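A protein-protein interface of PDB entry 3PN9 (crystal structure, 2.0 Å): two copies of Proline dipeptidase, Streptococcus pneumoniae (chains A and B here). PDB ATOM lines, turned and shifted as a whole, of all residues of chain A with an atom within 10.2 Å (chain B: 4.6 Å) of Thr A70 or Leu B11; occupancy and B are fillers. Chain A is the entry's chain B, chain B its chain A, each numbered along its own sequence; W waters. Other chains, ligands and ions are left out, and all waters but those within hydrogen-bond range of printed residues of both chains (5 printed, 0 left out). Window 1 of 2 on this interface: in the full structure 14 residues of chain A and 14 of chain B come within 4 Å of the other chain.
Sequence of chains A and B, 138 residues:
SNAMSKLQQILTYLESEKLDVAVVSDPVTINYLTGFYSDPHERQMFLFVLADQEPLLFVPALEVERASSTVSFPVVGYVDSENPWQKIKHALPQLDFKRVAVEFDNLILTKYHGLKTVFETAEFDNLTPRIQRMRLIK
Water W2 lies within hydrogen-bond range of O of Ala B51 (2.7 Å), O of Leu B11 (2.8 Å) and NH2 of Arg A66 (3.2 Å).
Water W3 lies within hydrogen-bond range of O of Ala B51 (2.7 Å), NE of Arg A66 (2.9 Å) and OG of Ser A69 (3.4 Å).
Water W4 lies within hydrogen-bond range of the side-chain amide oxygen of Asn A31 (2.8 Å), the backbone carbonyl oxygen of Gly A35 (2.8 Å), the side-chain amide nitrogen of Gln B8 (2.8 Å) and the backbone NH of Tyr A37 (3.3 Å).
Water W5 bridges OE1 of Glu B15 (2.8 Å) and NH1 of Arg A66 (2.8 Å).
Water W1 lies within hydrogen-bond range of OG1 of Thr B12 (2.9 Å), NH1 of Arg A66 (2.9 Å) and OE1 of Gln B8 (3.0 Å).
Position printed for both chains: 7.
Of the 10 pairs that touch across the chains among the printed residues, none has its exchanged pair printed and touching as well.
O of Gln B8 is in hydrogen-bond range of OG1 of Thr B12 (2.9 Å).
N of Asn A31 lies close to O of Phe A36 (3.5 Å).
The backbone NH (N) of Phe A36 sits at hydrogen-bond distance from the side-chain hydroxyl (OG1) of Thr A34 (3.1 Å).
O of Glu A65 is in hydrogen-bond range of OG of Ser A69 (3.0 Å).
O of Arg A66 lies within hydrogen-bond range of OG1 of Thr A70, 2.8 Å away.
Phe A36 touches Gln B8 (CA to NE2, 3.4 Å).
CD of Arg A66 touches CB of Leu B11, 3.7 Å away.
Arg A66 touches Thr B12 (NH1 to OG1, 3.8 Å).
Leu B7 touches Ser A69 (CD2 to O, 3.8 Å).
Ser A69 touches Leu B11.
Thr A70 touches Leu B7.
Thr A70 touches Leu B11.
The side-chain amide nitrogen of Gln B8 is in hydrogen-bond range of the backbone carbonyl oxygen of Gly A35, at 3.3 Å.
NE2 of Gln B8 sits close to N of Tyr A37 (2.8 Å).
NH2 of Arg A66 lies within salt-bridge range of OE1 of Glu B15 (2.8 Å).
Thr A70 touches two residues of chain B.
Of the printed residues of chain A, Leu B11 touches Arg A66, Ser A69 and Thr A70.
Gln B8 touches just these residues of chain A: Gly A35 (3.3 Å), Phe A36 (3.4 Å) and Tyr A37 (2.8 Å).
No residue of chain A comes within 4 Å of Ile B10.
Thr B12 touches just one residue of chain A: Arg A66.
No residue of chain A comes within 4 Å of Leu B14.
No residue of chain A comes within 4 Å of Ala B51.
Printed residues of chain B within 4 Å of Tyr A37: Gln B8 (2.8 Å).
Of the printed residues of chain A, Leu B7 touches Ser A69 and Thr A70.
Of the printed residues of chain B, Ser A69 touches Leu B7 and Leu B11.
Glu A63 touches none of the printed residues of chain B.
Val A75 touches none of the printed residues of chain B.
The nearest residue of chain B that does not touch Thr A70 is Gln B8 (4.3 Å).
The nearest printed residue of chain B that does not touch Phe A36 is Leu B11 (7.0 Å).
Of the 12 printed residues of chain B, 5 touch a printed residue of chain A.
Hydrophobic or aromatic side chains of chain B within 4 Å of the printed part of chain A: Leu B7 and Leu B11.
Among the printed residues, 10 pairs touch across the chains.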
ATOM      1  N   LEU A   7     -12.440 -17.039   2.842  1.00  0.00           N
ATOM      2  CA  LEU A   7     -12.490 -16.176   4.038  1.00  0.00           C
ATOM      3  C   LEU A   7     -13.471 -15.027   3.848  1.00  0.00           C
ATOM      4  O   LEU A   7     -14.173 -14.614   4.779  1.00  0.00           O
ATOM      5  CB  LEU A   7     -11.107 -15.622   4.375  1.00  0.00           C
ATOM      6  CG  LEU A   7     -10.111 -16.605   4.983  1.00  0.00           C
ATOM      7  CD1 LEU A   7      -8.625 -16.073   4.898  1.00  0.00           C
ATOM      8  CD2 LEU A   7     -10.464 -16.944   6.425  1.00  0.00           C
ATOM      9  N   ILE A  30      -9.271 -25.232   8.969  1.00  0.00           N
ATOM     10  CA  ILE A  30      -8.295 -24.164   8.853  1.00  0.00           C
ATOM     11  C   ILE A  30      -7.545 -24.246   7.524  1.00  0.00           C
ATOM     12  O   ILE A  30      -7.398 -23.245   6.809  1.00  0.00           O
ATOM     13  CB  ILE A  30      -7.256 -24.237  10.039  1.00  0.00           C
ATOM     14  CG1 ILE A  30      -8.108 -23.825  11.330  1.00  0.00           C
ATOM     15  CG2 ILE A  30      -6.159 -23.144   9.710  1.00  0.00           C
ATOM     16  CD1 ILE A  30      -7.268 -23.991  12.729  1.00  0.00           C
ATOM     17  N   ASN A  31      -7.143 -25.419   7.177  1.00  0.00           N
ATOM     18  CA  ASN A  31      -6.380 -25.623   5.898  1.00  0.00           C
ATOM     19  C   ASN A  31      -7.281 -25.309   4.680  1.00  0.00           C
ATOM     20  O   ASN A  31      -6.909 -24.543   3.776  1.00  0.00           O
ATOM     21  CB  ASN A  31      -5.888 -27.086   5.839  1.00  0.00           C
ATOM     22  CG  ASN A  31      -4.995 -27.327   4.606  1.00  0.00           C
ATOM     23  OD1 ASN A  31      -4.307 -26.413   4.143  1.00  0.00           O
ATOM     24  ND2 ASN A  31      -5.081 -28.504   4.050  1.00  0.00           N
ATOM     25  N   TYR A  32      -8.529 -25.790   4.731  1.00  0.00           N
ATOM     26  CA  TYR A  32      -9.525 -25.425   3.648  1.00  0.00           C
ATOM     27  C   TYR A  32      -9.663 -23.926   3.489  1.00  0.00           C
ATOM     28  O   TYR A  32      -9.707 -23.431   2.385  1.00  0.00           O
ATOM     29  CB  TYR A  32     -10.897 -26.014   4.044  1.00  0.00           C
ATOM     30  CG  TYR A  32     -12.028 -25.684   3.097  1.00  0.00           C
ATOM     31  CD1 TYR A  32     -11.988 -26.161   1.740  1.00  0.00           C
ATOM     32  CD2 TYR A  32     -13.088 -24.942   3.535  1.00  0.00           C
ATOM     33  CE1 TYR A  32     -13.051 -25.854   0.838  1.00  0.00           C
ATOM     34  CE2 TYR A  32     -14.187 -24.645   2.658  1.00  0.00           C
ATOM     35  CZ  TYR A  32     -14.115 -25.122   1.310  1.00  0.00           C
ATOM     36  OH  TYR A  32     -15.228 -24.818   0.530  1.00  0.00           O
ATOM     37  N   LEU A  33      -9.731 -23.149   4.583  1.00  0.00           N
ATOM     38  CA  LEU A  33      -9.940 -21.764   4.448  1.00  0.00           C
ATOM     39  C   LEU A  33      -8.642 -20.992   4.196  1.00  0.00           C
ATOM     40  O   LEU A  33      -8.742 -19.891   3.712  1.00  0.00           O
ATOM     41  CB  LEU A  33     -10.597 -21.146   5.736  1.00  0.00           C
ATOM     42  CG  LEU A  33     -11.991 -21.704   6.040  1.00  0.00           C
ATOM     43  CD1 LEU A  33     -12.502 -21.257   7.515  1.00  0.00           C
ATOM     44  CD2 LEU A  33     -13.043 -21.366   5.001  1.00  0.00           C
ATOM     45  N   THR A  34      -7.455 -21.493   4.579  1.00  0.00           N
ATOM     46  CA  THR A  34      -6.301 -20.572   4.556  1.00  0.00           C
ATOM     47  C   THR A  34      -5.137 -21.136   3.778  1.00  0.00           C
ATOM     48  O   THR A  34      -4.190 -20.401   3.548  1.00  0.00           O
ATOM     49  CB  THR A  34      -5.697 -20.280   6.022  1.00  0.00           C
ATOM     50  OG1 THR A  34      -5.238 -21.524   6.547  1.00  0.00           O
ATOM     51  CG2 THR A  34      -6.820 -19.673   6.962  1.00  0.00           C
ATOM     52  N   GLY A  35      -5.103 -22.435   3.539  1.00  0.00           N
ATOM     53  CA  GLY A  35      -3.905 -23.079   2.877  1.00  0.00           C
ATOM     54  C   GLY A  35      -2.797 -23.438   3.892  1.00  0.00           C
ATOM     55  O   GLY A  35      -1.787 -23.992   3.494  1.00  0.00           O
ATOM     56  N   PHE A  36      -3.067 -23.248   5.221  1.00  0.00           N
ATOM     57  CA  PHE A  36      -2.121 -23.667   6.231  1.00  0.00           C
ATOM     58  C   PHE A  36      -2.641 -24.931   6.959  1.00  0.00           C
ATOM     59  O   PHE A  36      -3.733 -24.925   7.561  1.00  0.00           O
ATOM     60  CB  PHE A  36      -1.909 -22.554   7.332  1.00  0.00           C
ATOM     61  CG  PHE A  36      -0.951 -22.998   8.380  1.00  0.00           C
ATOM     62  CD1 PHE A  36       0.393 -23.256   8.025  1.00  0.00           C
ATOM     63  CD2 PHE A  36      -1.380 -23.206   9.718  1.00  0.00           C
ATOM     64  CE1 PHE A  36       1.385 -23.742   9.003  1.00  0.00           C
ATOM     65  CE2 PHE A  36      -0.418 -23.689  10.686  1.00  0.00           C
ATOM     66  CZ  PHE A  36       0.906 -24.027  10.310  1.00  0.00           C
ATOM     67  N   TYR A  37      -1.838 -25.973   6.913  1.00  0.00           N
ATOM     68  CA  TYR A  37      -2.187 -27.235   7.579  1.00  0.00           C
ATOM     69  C   TYR A  37      -1.185 -27.526   8.696  1.00  0.00           C
ATOM     70  O   TYR A  37       0.054 -27.549   8.457  1.00  0.00           O
ATOM     71  CB  TYR A  37      -2.202 -28.440   6.570  1.00  0.00           C
ATOM     72  CG  TYR A  37      -2.498 -29.734   7.322  1.00  0.00           C
ATOM     73  CD1 TYR A  37      -3.810 -30.017   7.716  1.00  0.00           C
ATOM     74  CD2 TYR A  37      -1.435 -30.553   7.774  1.00  0.00           C
ATOM     75  CE1 TYR A  37      -4.117 -31.173   8.492  1.00  0.00           C
ATOM     76  CE2 TYR A  37      -1.686 -31.725   8.573  1.00  0.00           C
ATOM     77  CZ  TYR A  37      -3.033 -31.997   8.921  1.00  0.00           C
ATOM     78  OH  TYR A  37      -3.319 -33.092   9.681  1.00  0.00           O
ATOM     79  N   SER A  38      -1.664 -27.809   9.915  1.00  0.00           N
ATOM     80  CA  SER A  38      -0.756 -28.367  10.902  1.00  0.00           C
ATOM     81  C   SER A  38      -1.592 -29.268  11.824  1.00  0.00           C
ATOM     82  O   SER A  38      -2.757 -28.992  12.050  1.00  0.00           O
ATOM     83  CB  SER A  38      -0.227 -27.176  11.768  1.00  0.00           C
ATOM     84  OG  SER A  38       0.558 -27.685  12.848  1.00  0.00           O
ATOM     85  N   LEU A  57      -4.695 -15.862  12.821  1.00  0.00           N
ATOM     86  CA  LEU A  57      -4.438 -17.251  13.002  1.00  0.00           C
ATOM     87  C   LEU A  57      -3.536 -17.400  14.243  1.00  0.00           C
ATOM     88  O   LEU A  57      -2.471 -16.762  14.347  1.00  0.00           O
ATOM     89  CB  LEU A  57      -3.657 -17.786  11.782  1.00  0.00           C
ATOM     90  CG  LEU A  57      -3.209 -19.191  11.792  1.00  0.00           C
ATOM     91  CD1 LEU A  57      -4.324 -20.263  12.134  1.00  0.00           C
ATOM     92  CD2 LEU A  57      -2.588 -19.532  10.378  1.00  0.00           C
ATOM     93  N   VAL A  59      -1.408 -19.889  16.769  1.00  0.00           N
ATOM     94  CA  VAL A  59      -0.795 -21.192  16.609  1.00  0.00           C
ATOM     95  C   VAL A  59       0.255 -21.432  17.727  1.00  0.00           C
ATOM     96  O   VAL A  59       0.677 -20.474  18.332  1.00  0.00           O
ATOM     97  CB  VAL A  59      -0.009 -21.354  15.264  1.00  0.00           C
ATOM     98  CG1 VAL A  59      -1.004 -21.295  14.008  1.00  0.00           C
ATOM     99  CG2 VAL A  59       1.108 -20.247  15.136  1.00  0.00           C
ATOM    100  N   GLU A  63       5.120 -23.142  15.135  1.00  0.00           N
ATOM    101  CA  GLU A  63       4.477 -22.996  13.783  1.00  0.00           C
ATOM    102  C   GLU A  63       4.433 -21.558  13.270  1.00  0.00           C
ATOM    103  O   GLU A  63       3.986 -21.345  12.136  1.00  0.00           O
ATOM    104  CB  GLU A  63       3.050 -23.501  13.854  1.00  0.00           C
ATOM    105  CG  GLU A  63       2.985 -24.991  14.263  1.00  0.00           C
ATOM    106  CD  GLU A  63       3.256 -25.932  13.077  1.00  0.00           C
ATOM    107  OE1 GLU A  63       3.550 -25.501  11.918  1.00  0.00           O
ATOM    108  OE2 GLU A  63       3.156 -27.144  13.295  1.00  0.00           O
ATOM    109  N   VAL A  64       4.867 -20.557  14.043  1.00  0.00           N
ATOM    110  CA  VAL A  64       4.538 -19.183  13.650  1.00  0.00           C
ATOM    111  C   VAL A  64       5.242 -18.852  12.341  1.00  0.00           C
ATOM    112  O   VAL A  64       4.642 -18.191  11.475  1.00  0.00           O
ATOM    113  CB  VAL A  64       5.022 -18.126  14.699  1.00  0.00           C
ATOM    114  CG1 VAL A  64       4.969 -16.642  14.135  1.00  0.00           C
ATOM    115  CG2 VAL A  64       4.102 -18.174  15.955  1.00  0.00           C
ATOM    116  N   GLU A  65       6.512 -19.263  12.209  1.00  0.00           N
ATOM    117  CA  GLU A  65       7.224 -18.814  10.998  1.00  0.00           C
ATOM    118  C   GLU A  65       6.579 -19.472   9.707  1.00  0.00           C
ATOM    119  O   GLU A  65       6.390 -18.821   8.684  1.00  0.00           O
ATOM    120  CB  GLU A  65       8.677 -19.256  11.129  1.00  0.00           C
ATOM    121  CG  GLU A  65       9.501 -18.979   9.916  1.00  0.00           C
ATOM    122  CD  GLU A  65      11.061 -19.076  10.256  1.00  0.00           C
ATOM    123  OE1 GLU A  65      11.603 -20.201  10.411  1.00  0.00           O
ATOM    124  OE2 GLU A  65      11.701 -18.013  10.412  1.00  0.00           O
ATOM    125  N   ARG A  66       6.320 -20.775   9.750  1.00  0.00           N
ATOM    126  CA  ARG A  66       5.697 -21.474   8.595  1.00  0.00           C
ATOM    127  C   ARG A  66       4.314 -20.954   8.306  1.00  0.00           C
ATOM    128  O   ARG A  66       3.897 -20.715   7.163  1.00  0.00           O
ATOM    129  CB  ARG A  66       5.696 -23.026   8.899  1.00  0.00           C
ATOM    130  CG  ARG A  66       5.036 -23.905   7.804  1.00  0.00           C
ATOM    131  CD  ARG A  66       5.847 -23.830   6.472  1.00  0.00           C
ATOM    132  NE  ARG A  66       7.344 -23.850   6.642  1.00  0.00           N
ATOM    133  CZ  ARG A  66       8.099 -24.932   6.917  1.00  0.00           C
ATOM    134  NH1 ARG A  66       7.573 -26.125   7.089  1.00  0.00           N
ATOM    135  NH2 ARG A  66       9.412 -24.788   7.101  1.00  0.00           N
ATOM    136  N   ALA A  67       3.524 -20.731   9.337  1.00  0.00           N
ATOM    137  CA  ALA A  67       2.204 -20.185   9.143  1.00  0.00           C
ATOM    138  C   ALA A  67       2.249 -18.776   8.547  1.00  0.00           C
ATOM    139  O   ALA A  67       1.423 -18.456   7.653  1.00  0.00           O
ATOM    140  CB  ALA A  67       1.327 -20.077  10.509  1.00  0.00           C
ATOM    141  N   SER A  68       3.121 -17.932   9.093  1.00  0.00           N
ATOM    142  CA  SER A  68       3.284 -16.486   8.607  1.00  0.00           C
ATOM    143  C   SER A  68       3.721 -16.453   7.118  1.00  0.00           C
ATOM    144  O   SER A  68       3.401 -15.461   6.421  1.00  0.00           O
ATOM    145  CB  SER A  68       4.497 -15.825   9.402  1.00  0.00           C
ATOM    146  OG  SER A  68       4.041 -15.726  10.719  1.00  0.00           O
ATOM    147  N   SER A  69       4.465 -17.475   6.704  1.00  0.00           N
ATOM    148  CA  SER A  69       4.974 -17.560   5.310  1.00  0.00           C
ATOM    149  C   SER A  69       3.804 -18.045   4.418  1.00  0.00           C
ATOM    150  O   SER A  69       3.824 -17.848   3.215  1.00  0.00           O
ATOM    151  CB  SER A  69       6.047 -18.560   5.167  1.00  0.00           C
ATOM    152  OG  SER A  69       7.222 -18.142   5.928  1.00  0.00           O
ATOM    153  N   THR A  70       2.836 -18.704   5.025  1.00  0.00           N
ATOM    154  CA  THR A  70       1.766 -19.389   4.262  1.00  0.00           C
ATOM    155  C   THR A  70       0.646 -18.459   4.068  1.00  0.00           C
ATOM    156  O   THR A  70       0.043 -18.528   3.012  1.00  0.00           O
ATOM    157  CB  THR A  70       1.227 -20.650   4.971  1.00  0.00           C
ATOM    158  OG1 THR A  70       2.300 -21.549   5.058  1.00  0.00           O
ATOM    159  CG2 THR A  70       0.114 -21.356   4.199  1.00  0.00           C
ATOM    160  N   VAL A  71       0.247 -17.690   5.091  1.00  0.00           N
ATOM    161  CA  VAL A  71      -0.827 -16.764   4.982  1.00  0.00           C
ATOM    162  C   VAL A  71      -0.418 -15.302   4.956  1.00  0.00           C
ATOM    163  O   VAL A  71       0.645 -14.903   5.455  1.00  0.00           O
ATOM    164  CB  VAL A  71      -1.920 -16.914   6.127  1.00  0.00           C
ATOM    165  CG1 VAL A  71      -2.402 -18.378   6.178  1.00  0.00           C
ATOM    166  CG2 VAL A  71      -1.334 -16.520   7.565  1.00  0.00           C
ATOM    167  N   SER A  72      -1.309 -14.465   4.495  1.00  0.00           N
ATOM    168  CA  SER A  72      -0.953 -13.054   4.468  1.00  0.00           C
ATOM    169  C   SER A  72      -1.534 -12.179   5.592  1.00  0.00           C
ATOM    170  O   SER A  72      -1.123 -11.000   5.776  1.00  0.00           O
ATOM    171  CB  SER A  72      -1.341 -12.479   3.102  1.00  0.00           C
ATOM    172  OG  SER A  72      -2.628 -11.949   3.297  1.00  0.00           O
ATOM    173  N   PHE A  73      -2.370 -12.734   6.467  1.00  0.00           N
ATOM    174  CA  PHE A  73      -2.933 -11.881   7.518  1.00  0.00           C
ATOM    175  C   PHE A  73      -2.174 -12.219   8.840  1.00  0.00           C
ATOM    176  O   PHE A  73      -1.346 -13.152   8.855  1.00  0.00           O
ATOM    177  CB  PHE A  73      -4.472 -12.156   7.663  1.00  0.00           C
ATOM    178  CG  PHE A  73      -4.789 -13.610   7.689  1.00  0.00           C
ATOM    179  CD1 PHE A  73      -4.639 -14.337   8.901  1.00  0.00           C
ATOM    180  CD2 PHE A  73      -5.154 -14.287   6.500  1.00  0.00           C
ATOM    181  CE1 PHE A  73      -4.978 -15.707   8.974  1.00  0.00           C
ATOM    182  CE2 PHE A  73      -5.386 -15.694   6.545  1.00  0.00           C
ATOM    183  CZ  PHE A  73      -5.298 -16.409   7.796  1.00  0.00           C
ATOM    184  N   PRO A  74      -2.505 -11.556   9.936  1.00  0.00           N
ATOM    185  CA  PRO A  74      -1.629 -11.727  11.124  1.00  0.00           C
ATOM    186  C   PRO A  74      -1.649 -13.142  11.770  1.00  0.00           C
ATOM    187  O   PRO A  74      -2.711 -13.778  11.809  1.00  0.00           O
ATOM    188  CB  PRO A  74      -2.248 -10.704  12.122  1.00  0.00           C
ATOM    189  CG  PRO A  74      -2.730  -9.577  11.233  1.00  0.00           C
ATOM    190  CD  PRO A  74      -3.448 -10.429  10.146  1.00  0.00           C
ATOM    191  N   VAL A  75      -0.491 -13.601  12.258  1.00  0.00           N
ATOM    192  CA  VAL A  75      -0.349 -14.843  12.947  1.00  0.00           C
ATOM    193  C   VAL A  75       0.234 -14.524  14.343  1.00  0.00           C
ATOM    194  O   VAL A  75       1.193 -13.750  14.414  1.00  0.00           O
ATOM    195  CB  VAL A  75       0.640 -15.744  12.186  1.00  0.00           C
ATOM    196  CG1 VAL A  75       0.965 -17.005  13.018  1.00  0.00           C
ATOM    197  CG2 VAL A  75       0.051 -16.129  10.734  1.00  0.00           C
ATOM    198  N   LEU B   7       1.711 -24.568  -1.997  1.00  0.00           N
ATOM    199  CA  LEU B   7       2.747 -23.605  -1.522  1.00  0.00           C
ATOM    200  C   LEU B   7       3.331 -24.148  -0.218  1.00  0.00           C
ATOM    201  O   LEU B   7       4.523 -24.092  -0.015  1.00  0.00           O
ATOM    202  CB  LEU B   7       2.111 -22.218  -1.278  1.00  0.00           C
ATOM    203  CG  LEU B   7       2.825 -21.283  -0.205  1.00  0.00           C
ATOM    204  CD1 LEU B   7       4.286 -21.089  -0.708  1.00  0.00           C
ATOM    205  CD2 LEU B   7       2.269 -19.793   0.399  1.00  0.00           C
ATOM    206  N   GLN B   8       2.488 -24.630   0.687  1.00  0.00           N
ATOM    207  CA  GLN B   8       3.078 -25.124   1.923  1.00  0.00           C
ATOM    208  C   GLN B   8       3.987 -26.383   1.698  1.00  0.00           C
ATOM    209  O   GLN B   8       5.039 -26.580   2.373  1.00  0.00           O
ATOM    210  CB  GLN B   8       1.983 -25.406   2.983  1.00  0.00           C
ATOM    211  CG  GLN B   8       2.646 -25.747   4.373  1.00  0.00           C
ATOM    212  CD  GLN B   8       1.641 -25.937   5.551  1.00  0.00           C
ATOM    213  OE1 GLN B   8       2.023 -26.479   6.634  1.00  0.00           O
ATOM    214  NE2 GLN B   8       0.389 -25.678   5.286  1.00  0.00           N
ATOM    215  N   GLN B   9       3.638 -27.226   0.714  1.00  0.00           N
ATOM    216  CA  GLN B   9       4.518 -28.372   0.394  1.00  0.00           C
ATOM    217  C   GLN B   9       5.858 -27.836  -0.107  1.00  0.00           C
ATOM    218  O   GLN B   9       6.892 -28.425   0.188  1.00  0.00           O
ATOM    219  CB  GLN B   9       3.928 -29.132  -0.791  1.00  0.00           C
ATOM    220  CG  GLN B   9       2.763 -30.105  -0.286  1.00  0.00           C
ATOM    221  CD  GLN B   9       2.312 -31.046  -1.425  1.00  0.00           C
ATOM    222  OE1 GLN B   9       3.148 -31.837  -1.965  1.00  0.00           O
ATOM    223  NE2 GLN B   9       1.043 -30.912  -1.842  1.00  0.00           N
ATOM    224  N   ILE B  10       5.871 -26.763  -0.935  1.00  0.00           N
ATOM    225  CA  ILE B  10       7.220 -26.258  -1.329  1.00  0.00           C
ATOM    226  C   ILE B  10       7.921 -25.680  -0.127  1.00  0.00           C
ATOM    227  O   ILE B  10       9.138 -25.909   0.030  1.00  0.00           O
ATOM    228  CB  ILE B  10       7.046 -25.159  -2.432  1.00  0.00           C
ATOM    229  CG1 ILE B  10       6.590 -25.881  -3.723  1.00  0.00           C
ATOM    230  CG2 ILE B  10       8.451 -24.407  -2.650  1.00  0.00           C
ATOM    231  CD1 ILE B  10       6.172 -24.968  -4.799  1.00  0.00           C
ATOM    232  N   LEU B  11       7.194 -24.982   0.777  1.00  0.00           N
ATOM    233  CA  LEU B  11       7.942 -24.502   2.003  1.00  0.00           C
ATOM    234  C   LEU B  11       8.575 -25.622   2.759  1.00  0.00           C
ATOM    235  O   LEU B  11       9.691 -25.492   3.352  1.00  0.00           O
ATOM    236  CB  LEU B  11       6.996 -23.680   2.978  1.00  0.00           C
ATOM    237  CG  LEU B  11       6.414 -22.398   2.334  1.00  0.00           C
ATOM    238  CD1 LEU B  11       5.289 -21.679   3.265  1.00  0.00           C
ATOM    239  CD2 LEU B  11       7.562 -21.409   2.136  1.00  0.00           C
ATOM    240  N   THR B  12       7.824 -26.714   2.879  1.00  0.00           N
ATOM    241  CA  THR B  12       8.337 -27.842   3.659  1.00  0.00           C
ATOM    242  C   THR B  12       9.580 -28.382   2.971  1.00  0.00           C
ATOM    243  O   THR B  12      10.577 -28.807   3.612  1.00  0.00           O
ATOM    244  CB  THR B  12       7.184 -28.955   3.721  1.00  0.00           C
ATOM    245  OG1 THR B  12       6.063 -28.364   4.416  1.00  0.00           O
ATOM    246  CG2 THR B  12       7.606 -30.166   4.461  1.00  0.00           C
ATOM    247  N   TYR B  13       9.506 -28.482   1.644  1.00  0.00           N
ATOM    248  CA  TYR B  13      10.620 -29.010   0.845  1.00  0.00           C
ATOM    249  C   TYR B  13      11.895 -28.100   0.953  1.00  0.00           C
ATOM    250  O   TYR B  13      13.022 -28.619   1.070  1.00  0.00           O
ATOM    251  CB  TYR B  13      10.150 -29.050  -0.624  1.00  0.00           C
ATOM    252  CG  TYR B  13      11.200 -29.386  -1.667  1.00  0.00           C
ATOM    253  CD1 TYR B  13      11.581 -30.735  -1.744  1.00  0.00           C
ATOM    254  CD2 TYR B  13      11.776 -28.438  -2.551  1.00  0.00           C
ATOM    255  CE1 TYR B  13      12.463 -31.176  -2.606  1.00  0.00           C
ATOM    256  CE2 TYR B  13      12.750 -28.912  -3.536  1.00  0.00           C
ATOM    257  CZ  TYR B  13      13.067 -30.280  -3.507  1.00  0.00           C
ATOM    258  OH  TYR B  13      13.922 -31.068  -4.346  1.00  0.00           O
ATOM    259  N   LEU B  14      11.692 -26.752   1.002  1.00  0.00           N
ATOM    260  CA  LEU B  14      12.828 -25.843   1.118  1.00  0.00           C
ATOM    261  C   LEU B  14      13.538 -26.162   2.444  1.00  0.00           C
ATOM    262  O   LEU B  14      14.784 -26.192   2.517  1.00  0.00           O
ATOM    263  CB  LEU B  14      12.375 -24.357   1.106  1.00  0.00           C
ATOM    264  CG  LEU B  14      11.691 -23.959  -0.231  1.00  0.00           C
ATOM    265  CD1 LEU B  14      11.230 -22.470  -0.149  1.00  0.00           C
ATOM    266  CD2 LEU B  14      12.685 -24.128  -1.424  1.00  0.00           C
ATOM    267  N   GLU B  15      12.761 -26.387   3.511  1.00  0.00           N
ATOM    268  CA  GLU B  15      13.437 -26.680   4.764  1.00  0.00           C
ATOM    269  C   GLU B  15      14.198 -28.035   4.709  1.00  0.00           C
ATOM    270  O   GLU B  15      15.363 -28.110   5.141  1.00  0.00           O
ATOM    271  CB  GLU B  15      12.426 -26.667   5.932  1.00  0.00           C
ATOM    272  CG  GLU B  15      13.087 -27.235   7.221  1.00  0.00           C
ATOM    273  CD  GLU B  15      12.182 -27.104   8.453  1.00  0.00           C
ATOM    274  OE1 GLU B  15      10.984 -26.721   8.346  1.00  0.00           O
ATOM    275  OE2 GLU B  15      12.670 -27.404   9.541  1.00  0.00           O
ATOM    276  N   VAL B  49       9.576 -18.604  -4.208  1.00  0.00           N
ATOM    277  CA  VAL B  49       9.010 -19.132  -2.935  1.00  0.00           C
ATOM    278  C   VAL B  49      10.204 -19.130  -1.993  1.00  0.00           C
ATOM    279  O   VAL B  49      11.166 -19.860  -2.197  1.00  0.00           O
ATOM    280  CB  VAL B  49       8.479 -20.587  -3.091  1.00  0.00           C
ATOM    281  CG1 VAL B  49       7.754 -20.988  -1.740  1.00  0.00           C
ATOM    282  CG2 VAL B  49       7.402 -20.652  -4.273  1.00  0.00           C
ATOM    283  N   LEU B  50      10.146 -18.247  -1.024  1.00  0.00           N
ATOM    284  CA  LEU B  50      11.214 -18.058  -0.098  1.00  0.00           C
ATOM    285  C   LEU B  50      11.019 -19.022   1.096  1.00  0.00           C
ATOM    286  O   LEU B  50       9.884 -19.347   1.412  1.00  0.00           O
ATOM    287  CB  LEU B  50      11.079 -16.606   0.468  1.00  0.00           C
ATOM    288  CG  LEU B  50      11.449 -15.562  -0.669  1.00  0.00           C
ATOM    289  CD1 LEU B  50      10.900 -14.114  -0.376  1.00  0.00           C
ATOM    290  CD2 LEU B  50      13.015 -15.527  -0.725  1.00  0.00           C
ATOM    291  N   ALA B  51      12.106 -19.362   1.806  1.00  0.00           N
ATOM    292  CA  ALA B  51      12.010 -20.428   2.825  1.00  0.00           C
ATOM    293  C   ALA B  51      11.206 -19.930   3.999  1.00  0.00           C
ATOM    294  O   ALA B  51      10.436 -20.718   4.591  1.00  0.00           O
ATOM    295  CB  ALA B  51      13.390 -20.861   3.334  1.00  0.00           C
HETATM  296  O   HOH W   1       4.949 -27.291   6.838  1.00  0.00           O
HETATM  297  O   HOH W   2      10.846 -23.344   4.652  1.00  0.00           O
HETATM  298  O   HOH W   3       8.535 -21.243   6.399  1.00  0.00           O
HETATM  299  O   HOH W   4      -1.609 -26.761   3.681  1.00  0.00           O
HETATM  300  O   HOH W   5       8.978 -28.512   7.687  1.00  0.00           O
